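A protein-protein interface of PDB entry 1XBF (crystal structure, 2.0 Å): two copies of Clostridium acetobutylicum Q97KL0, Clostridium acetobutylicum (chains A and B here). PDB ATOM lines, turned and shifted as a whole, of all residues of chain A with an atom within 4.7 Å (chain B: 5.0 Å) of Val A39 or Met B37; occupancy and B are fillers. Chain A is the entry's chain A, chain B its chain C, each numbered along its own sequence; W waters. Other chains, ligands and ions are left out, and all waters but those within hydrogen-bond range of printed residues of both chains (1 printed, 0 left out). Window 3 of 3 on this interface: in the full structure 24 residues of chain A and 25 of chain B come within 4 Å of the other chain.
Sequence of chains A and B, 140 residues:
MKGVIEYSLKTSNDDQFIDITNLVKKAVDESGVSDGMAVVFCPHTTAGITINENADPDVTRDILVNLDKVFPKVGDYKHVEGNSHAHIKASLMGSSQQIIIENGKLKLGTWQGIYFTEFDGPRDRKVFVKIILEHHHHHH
The side-chain amide oxygen (OE1) of Gln A98 sits close to the side-chain amide oxygen (OE1) of Gln B98 (3.0 Å).
O of Met A37 sits at hydrogen-bond distance from N of Ile A132. O of Lys A130 is in hydrogen-bond range of N of Val A39 (2.8 Å). N of Phe A41 sits at hydrogen-bond distance from O of Phe A128 (2.8 Å). The backbone NH of Ile B101 lies within hydrogen-bond range of the backbone carbonyl oxygen of Gly B36. The backbone NH (N) of Ile B132 is in hydrogen-bond range of the backbone carbonyl oxygen (O) of Met B37, at 2.7 Å.
Among the printed residues, pairs that only touch across the chains: Lys A130 with Gly B36 (3.3 Å), Val A39 with Met B37 (3.3 Å), Phe A41 with Gln B98 (3.4 Å), Ile A132 with Met B37 (3.4 Å), Lys A130 with Met B37 (3.5 Å), Lys A130 with Ile B100 (3.7 Å), Val A39 with Gln B98 (3.7 Å), Phe A128 with Ile B100 (3.8 Å) and Phe A41 with Ile B100 (3.98 Å).
Of the printed residues of chain B, Gln A98 touches Gln B98. Of the printed residues of chain B, Phe A128 touches Ile B100 (3.8 Å). Printed residues of chain B within 4 Å of Lys A130: Gly B36 (3.3 Å), Met B37 (3.5 Å) and Ile B100 (3.7 Å). Printed residues of chain A within 4 Å of Gly B36: Lys A130 (3.3 Å). Of chain A, only Val A39 (3.3 Å), Lys A130 (3.5 Å) and Ile A132 (3.4 Å) come within 4 Å of Met B37. Val B39 touches none of the printed residues of chain A. Of the printed residues of chain A, Ile B100 touches Phe A41 (3.98 Å), Phe A128 (3.8 Å) and Lys A130 (3.7 Å). The nearest residue of chain B that does not touch Val A39 is Ile B100 (4.7 Å).
Printed residues of chain A that touch a printed residue of chain B: Val A39, Phe A41, Gln A98, Phe A128, Lys A130 and Ile A132. Along chain A the printed residues that touch a printed residue of chain B span positions 39 to 132. Among the printed residues, 10 pairs touch across the chains.
Val A39 touches Met B37, but with the chains exchanged Met A37 does not touch Val B39 (9.3 Å). Gln A98 touches its own counterpart, Gln B98. Lys A130 touches Met B37, but with the chains exchanged Met A37 does not touch Lys B130 (12.7 Å). Ile A132 touches Met B37, but with the chains exchanged Met A37 does not touch Ile B132 (8.4 Å). 6 positions are printed for both chains.
Water W1 lies within hydrogen-bond range of the backbone carbonyl oxygen (O) of Ile B101, the side-chain carboxylate (OD2) of Asp B35 and the side-chain amino group (NZ) of Lys A130.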
ATOM      1  N   MET A  37      24.181 -29.707  20.685  1.00  0.00           N
ATOM      2  CA  MET A  37      23.111 -30.090  21.593  1.00  0.00           C
ATOM      3  C   MET A  37      21.756 -29.974  20.919  1.00  0.00           C
ATOM      4  O   MET A  37      21.538 -29.088  20.101  1.00  0.00           O
ATOM      5  CB  MET A  37      23.116 -29.180  22.828  1.00  0.00           C
ATOM      6  CG  MET A  37      24.300 -29.354  23.771  1.00  0.00           C
ATOM      7  SD  MET A  37      24.180 -30.969  24.836  1.00  0.00           S
ATOM      8  CE  MET A  37      22.542 -30.580  25.766  1.00  0.00           C
ATOM      9  N   ALA A  38      20.848 -30.877  21.268  1.00  0.00           N
ATOM     10  CA  ALA A  38      19.495 -30.844  20.732  1.00  0.00           C
ATOM     11  C   ALA A  38      18.577 -30.561  21.908  1.00  0.00           C
ATOM     12  O   ALA A  38      18.492 -31.357  22.844  1.00  0.00           O
ATOM     13  CB  ALA A  38      19.133 -32.177  20.098  1.00  0.00           C
ATOM     14  N   VAL A  39      17.911 -29.417  21.875  1.00  0.00           N
ATOM     15  CA  VAL A  39      16.996 -29.063  22.943  1.00  0.00           C
ATOM     16  C   VAL A  39      15.566 -29.259  22.458  1.00  0.00           C
ATOM     17  O   VAL A  39      15.174 -28.719  21.421  1.00  0.00           O
ATOM     18  CB  VAL A  39      17.193 -27.597  23.388  1.00  0.00           C
ATOM     19  CG1 VAL A  39      16.125 -27.211  24.396  1.00  0.00           C
ATOM     20  CG2 VAL A  39      18.572 -27.424  23.998  1.00  0.00           C
ATOM     21  N   VAL A  40      14.796 -30.051  23.201  1.00  0.00           N
ATOM     22  CA  VAL A  40      13.406 -30.321  22.868  1.00  0.00           C
ATOM     23  C   VAL A  40      12.545 -29.616  23.914  1.00  0.00           C
ATOM     24  O   VAL A  40      12.620 -29.920  25.109  1.00  0.00           O
ATOM     25  CB  VAL A  40      13.117 -31.837  22.881  1.00  0.00           C
ATOM     26  CG1 VAL A  40      11.723 -32.109  22.321  1.00  0.00           C
ATOM     27  CG2 VAL A  40      14.176 -32.575  22.057  1.00  0.00           C
ATOM     28  N   PHE A  41      11.739 -28.664  23.463  1.00  0.00           N
ATOM     29  CA  PHE A  41      10.906 -27.894  24.368  1.00  0.00           C
ATOM     30  C   PHE A  41       9.421 -28.048  24.084  1.00  0.00           C
ATOM     31  O   PHE A  41       8.985 -28.037  22.928  1.00  0.00           O
ATOM     32  CB  PHE A  41      11.321 -26.422  24.293  1.00  0.00           C
ATOM     33  CG  PHE A  41      10.621 -25.539  25.272  1.00  0.00           C
ATOM     34  CD1 PHE A  41       9.324 -25.089  25.030  1.00  0.00           C
ATOM     35  CD2 PHE A  41      11.252 -25.163  26.456  1.00  0.00           C
ATOM     36  CE1 PHE A  41       8.664 -24.279  25.952  1.00  0.00           C
ATOM     37  CE2 PHE A  41      10.604 -24.356  27.386  1.00  0.00           C
ATOM     38  CZ  PHE A  41       9.308 -23.911  27.137  1.00  0.00           C
ATOM     39  N   GLN A  97      13.941 -31.283  27.555  1.00  0.00           N
ATOM     40  CA  GLN A  97      14.992 -32.249  27.813  1.00  0.00           C
ATOM     41  C   GLN A  97      16.010 -31.974  26.723  1.00  0.00           C
ATOM     42  O   GLN A  97      15.647 -31.508  25.649  1.00  0.00           O
ATOM     43  CB  GLN A  97      14.467 -33.688  27.691  1.00  0.00           C
ATOM     44  CG  GLN A  97      13.321 -34.048  28.647  1.00  0.00           C
ATOM     45  CD  GLN A  97      13.698 -33.932  30.114  1.00  0.00           C
ATOM     46  OE1 GLN A  97      12.826 -33.943  30.997  1.00  0.00           O
ATOM     47  NE2 GLN A  97      14.993 -33.828  30.389  1.00  0.00           N
ATOM     48  N   GLN A  98      17.280 -32.230  26.996  1.00  0.00           N
ATOM     49  CA  GLN A  98      18.292 -32.005  25.981  1.00  0.00           C
ATOM     50  C   GLN A  98      19.090 -33.271  25.760  1.00  0.00           C
ATOM     51  O   GLN A  98      19.264 -34.075  26.678  1.00  0.00           O
ATOM     52  CB  GLN A  98      19.214 -30.841  26.364  1.00  0.00           C
ATOM     53  CG  GLN A  98      19.650 -30.800  27.811  1.00  0.00           C
ATOM     54  CD  GLN A  98      20.611 -29.654  28.086  1.00  0.00           C
ATOM     55  OE1 GLN A  98      20.591 -28.629  27.400  1.00  0.00           O
ATOM     56  NE2 GLN A  98      21.447 -29.817  29.100  1.00  0.00           N
ATOM     57  N   PHE A 128       8.998 -27.742  20.148  1.00  0.00           N
ATOM     58  CA  PHE A 128      10.085 -26.980  19.549  1.00  0.00           C
ATOM     59  C   PHE A 128      11.393 -27.743  19.676  1.00  0.00           C
ATOM     60  O   PHE A 128      11.670 -28.351  20.712  1.00  0.00           O
ATOM     61  CB  PHE A 128      10.262 -25.620  20.230  1.00  0.00           C
ATOM     62  CG  PHE A 128       8.994 -24.836  20.394  1.00  0.00           C
ATOM     63  CD1 PHE A 128       7.950 -24.956  19.485  1.00  0.00           C
ATOM     64  CD2 PHE A 128       8.869 -23.928  21.441  1.00  0.00           C
ATOM     65  CE1 PHE A 128       6.799 -24.178  19.612  1.00  0.00           C
ATOM     66  CE2 PHE A 128       7.726 -23.142  21.582  1.00  0.00           C
ATOM     67  CZ  PHE A 128       6.685 -23.266  20.665  1.00  0.00           C
ATOM     68  N   VAL A 129      12.197 -27.706  18.620  1.00  0.00           N
ATOM     69  CA  VAL A 129      13.482 -28.382  18.623  1.00  0.00           C
ATOM     70  C   VAL A 129      14.559 -27.389  18.205  1.00  0.00           C
ATOM     71  O   VAL A 129      14.513 -26.836  17.105  1.00  0.00           O
ATOM     72  CB  VAL A 129      13.495 -29.579  17.646  1.00  0.00           C
ATOM     73  CG1 VAL A 129      14.827 -30.298  17.721  1.00  0.00           C
ATOM     74  CG2 VAL A 129      12.358 -30.532  17.982  1.00  0.00           C
ATOM     75  N   LYS A 130      15.516 -27.141  19.091  1.00  0.00           N
ATOM     76  CA  LYS A 130      16.594 -26.218  18.771  1.00  0.00           C
ATOM     77  C   LYS A 130      17.919 -26.964  18.779  1.00  0.00           C
ATOM     78  O   LYS A 130      18.258 -27.641  19.751  1.00  0.00           O
ATOM     79  CB  LYS A 130      16.629 -25.061  19.773  1.00  0.00           C
ATOM     80  CG  LYS A 130      17.639 -23.971  19.426  1.00  0.00           C
ATOM     81  CD  LYS A 130      17.471 -22.750  20.321  1.00  0.00           C
ATOM     82  CE  LYS A 130      18.413 -21.619  19.908  1.00  0.00           C
ATOM     83  NZ  LYS A 130      18.102 -21.083  18.549  1.00  0.00           N
ATOM     84  N   ILE A 132      21.830 -26.732  18.888  1.00  0.00           N
ATOM     85  CA  ILE A 132      22.913 -25.829  19.268  1.00  0.00           C
ATOM     86  C   ILE A 132      24.225 -26.328  18.678  1.00  0.00           C
ATOM     87  O   ILE A 132      24.811 -27.292  19.169  1.00  0.00           O
ATOM     88  CB  ILE A 132      23.052 -25.729  20.799  1.00  0.00           C
ATOM     89  CG1 ILE A 132      21.742 -25.220  21.401  1.00  0.00           C
ATOM     90  CG2 ILE A 132      24.192 -24.788  21.162  1.00  0.00           C
ATOM     91  CD1 ILE A 132      21.302 -23.877  20.857  1.00  0.00           C
ATOM     92  N   ASP B  35      19.053 -14.753  19.360  1.00  0.00           N
ATOM     93  CA  ASP B  35      18.761 -16.178  19.292  1.00  0.00           C
ATOM     94  C   ASP B  35      19.766 -16.930  20.140  1.00  0.00           C
ATOM     95  O   ASP B  35      20.976 -16.843  19.920  1.00  0.00           O
ATOM     96  CB  ASP B  35      18.823 -16.682  17.851  1.00  0.00           C
ATOM     97  CG  ASP B  35      17.592 -16.310  17.055  1.00  0.00           C
ATOM     98  OD1 ASP B  35      17.382 -15.102  16.818  1.00  0.00           O
ATOM     99  OD2 ASP B  35      16.834 -17.228  16.677  1.00  0.00           O
ATOM    100  N   GLY B  36      19.257 -17.665  21.120  1.00  0.00           N
ATOM    101  CA  GLY B  36      20.133 -18.419  21.991  1.00  0.00           C
ATOM    102  C   GLY B  36      19.344 -19.258  22.967  1.00  0.00           C
ATOM    103  O   GLY B  36      18.261 -19.746  22.648  1.00  0.00           O
ATOM    104  N   MET B  37      19.887 -19.412  24.167  1.00  0.00           N
ATOM    105  CA  MET B  37      19.234 -20.207  25.194  1.00  0.00           C
ATOM    106  C   MET B  37      19.329 -19.511  26.545  1.00  0.00           C
ATOM    107  O   MET B  37      20.384 -18.985  26.911  1.00  0.00           O
ATOM    108  CB  MET B  37      19.913 -21.578  25.292  1.00  0.00           C
ATOM    109  CG  MET B  37      18.992 -22.700  25.714  1.00  0.00           C
ATOM    110  SD  MET B  37      17.731 -23.063  24.306  1.00  0.00           S
ATOM    111  CE  MET B  37      18.843 -24.187  23.211  1.00  0.00           C
ATOM    112  N   ALA B  38      18.224 -19.498  27.281  1.00  0.00           N
ATOM    113  CA  ALA B  38      18.207 -18.903  28.606  1.00  0.00           C
ATOM    114  C   ALA B  38      18.136 -20.058  29.600  1.00  0.00           C
ATOM    115  O   ALA B  38      17.176 -20.831  29.592  1.00  0.00           O
ATOM    116  CB  ALA B  38      16.993 -17.991  28.768  1.00  0.00           C
ATOM    117  N   VAL B  39      19.169 -20.197  30.424  1.00  0.00           N
ATOM    118  CA  VAL B  39      19.207 -21.251  31.430  1.00  0.00           C
ATOM    119  C   VAL B  39      18.929 -20.599  32.780  1.00  0.00           C
ATOM    120  O   VAL B  39      19.626 -19.661  33.176  1.00  0.00           O
ATOM    121  CB  VAL B  39      20.587 -21.928  31.493  1.00  0.00           C
ATOM    122  CG1 VAL B  39      20.603 -22.963  32.612  1.00  0.00           C
ATOM    123  CG2 VAL B  39      20.910 -22.575  30.173  1.00  0.00           C
ATOM    124  N   GLN B  98      15.286 -24.694  30.925  1.00  0.00           N
ATOM    125  CA  GLN B  98      15.839 -24.034  29.746  1.00  0.00           C
ATOM    126  C   GLN B  98      14.741 -23.446  28.884  1.00  0.00           C
ATOM    127  O   GLN B  98      13.694 -24.063  28.699  1.00  0.00           O
ATOM    128  CB  GLN B  98      16.629 -25.053  28.923  1.00  0.00           C
ATOM    129  CG  GLN B  98      18.061 -24.683  28.651  1.00  0.00           C
ATOM    130  CD  GLN B  98      18.826 -25.812  27.981  1.00  0.00           C
ATOM    131  OE1 GLN B  98      20.029 -25.707  27.743  1.00  0.00           O
ATOM    132  NE2 GLN B  98      18.126 -26.901  27.677  1.00  0.00           N
ATOM    133  N   ILE B  99      14.982 -22.251  28.347  1.00  0.00           N
ATOM    134  CA  ILE B  99      14.013 -21.598  27.490  1.00  0.00           C
ATOM    135  C   ILE B  99      14.658 -21.090  26.193  1.00  0.00           C
ATOM    136  O   ILE B  99      15.704 -20.442  26.209  1.00  0.00           O
ATOM    137  CB  ILE B  99      13.321 -20.414  28.198  1.00  0.00           C
ATOM    138  CG1 ILE B  99      12.742 -20.845  29.557  1.00  0.00           C
ATOM    139  CG2 ILE B  99      12.181 -19.915  27.333  1.00  0.00           C
ATOM    140  CD1 ILE B  99      13.714 -20.750  30.730  1.00  0.00           C
ATOM    141  N   ILE B 100      14.026 -21.394  25.069  1.00  0.00           N
ATOM    142  CA  ILE B 100      14.556 -20.971  23.784  1.00  0.00           C
ATOM    143  C   ILE B 100      14.394 -19.467  23.585  1.00  0.00           C
ATOM    144  O   ILE B 100      13.335 -18.902  23.862  1.00  0.00           O
ATOM    145  CB  ILE B 100      13.856 -21.733  22.633  1.00  0.00           C
ATOM    146  CG1 ILE B 100      14.191 -23.223  22.746  1.00  0.00           C
ATOM    147  CG2 ILE B 100      14.300 -21.185  21.274  1.00  0.00           C
ATOM    148  CD1 ILE B 100      13.414 -24.111  21.819  1.00  0.00           C
ATOM    149  N   ILE B 101      15.468 -18.820  23.144  1.00  0.00           N
ATOM    150  CA  ILE B 101      15.433 -17.389  22.868  1.00  0.00           C
ATOM    151  C   ILE B 101      15.340 -17.252  21.357  1.00  0.00           C
ATOM    152  O   ILE B 101      16.184 -17.766  20.624  1.00  0.00           O
ATOM    153  CB  ILE B 101      16.706 -16.668  23.347  1.00  0.00           C
ATOM    154  CG1 ILE B 101      16.856 -16.810  24.861  1.00  0.00           C
ATOM    155  CG2 ILE B 101      16.631 -15.184  22.971  1.00  0.00           C
ATOM    156  CD1 ILE B 101      18.157 -16.248  25.399  1.00  0.00           C
ATOM    157  N   LYS B 130      21.655 -17.552  32.971  1.00  0.00           N
ATOM    158  CA  LYS B 130      22.767 -17.520  32.027  1.00  0.00           C
ATOM    159  C   LYS B 130      22.223 -17.574  30.602  1.00  0.00           C
ATOM    160  O   LYS B 130      21.461 -18.478  30.256  1.00  0.00           O
ATOM    161  CB  LYS B 130      23.689 -18.719  32.282  1.00  0.00           C
ATOM    162  CG  LYS B 130      25.163 -18.522  31.922  1.00  0.00           C
ATOM    163  CD  LYS B 130      25.395 -18.376  30.428  1.00  0.00           C
ATOM    164  CE  LYS B 130      26.864 -18.613  30.065  1.00  0.00           C
ATOM    165  NZ  LYS B 130      27.802 -17.710  30.785  1.00  0.00           N
ATOM    166  N   ILE B 131      22.599 -16.595  29.785  1.00  0.00           N
ATOM    167  CA  ILE B 131      22.159 -16.544  28.394  1.00  0.00           C
ATOM    168  C   ILE B 131      23.261 -17.187  27.553  1.00  0.00           C
ATOM    169  O   ILE B 131      24.430 -16.815  27.669  1.00  0.00           O
ATOM    170  CB  ILE B 131      21.947 -15.084  27.933  1.00  0.00           C
ATOM    171  CG1 ILE B 131      20.990 -14.365  28.891  1.00  0.00           C
ATOM    172  CG2 ILE B 131      21.413 -15.055  26.510  1.00  0.00           C
ATOM    173  CD1 ILE B 131      19.565 -14.897  28.898  1.00  0.00           C
ATOM    174  N   ILE B 132      22.900 -18.151  26.709  1.00  0.00           N
ATOM    175  CA  ILE B 132      23.896 -18.847  25.895  1.00  0.00           C
ATOM    176  C   ILE B 132      23.774 -18.599  24.387  1.00  0.00           C
ATOM    177  O   ILE B 132      22.680 -18.351  23.872  1.00  0.00           O
ATOM    178  CB  ILE B 132      23.832 -20.376  26.135  1.00  0.00           C
ATOM    179  CG1 ILE B 132      23.862 -20.677  27.636  1.00  0.00           C
ATOM    180  CG2 ILE B 132      25.015 -21.057  25.452  1.00  0.00           C
ATOM    181  CD1 ILE B 132      23.621 -22.139  27.974  1.00  0.00           C
HETATM  182  O   HOH W   1      15.750 -19.312  18.410  1.00  0.00           O
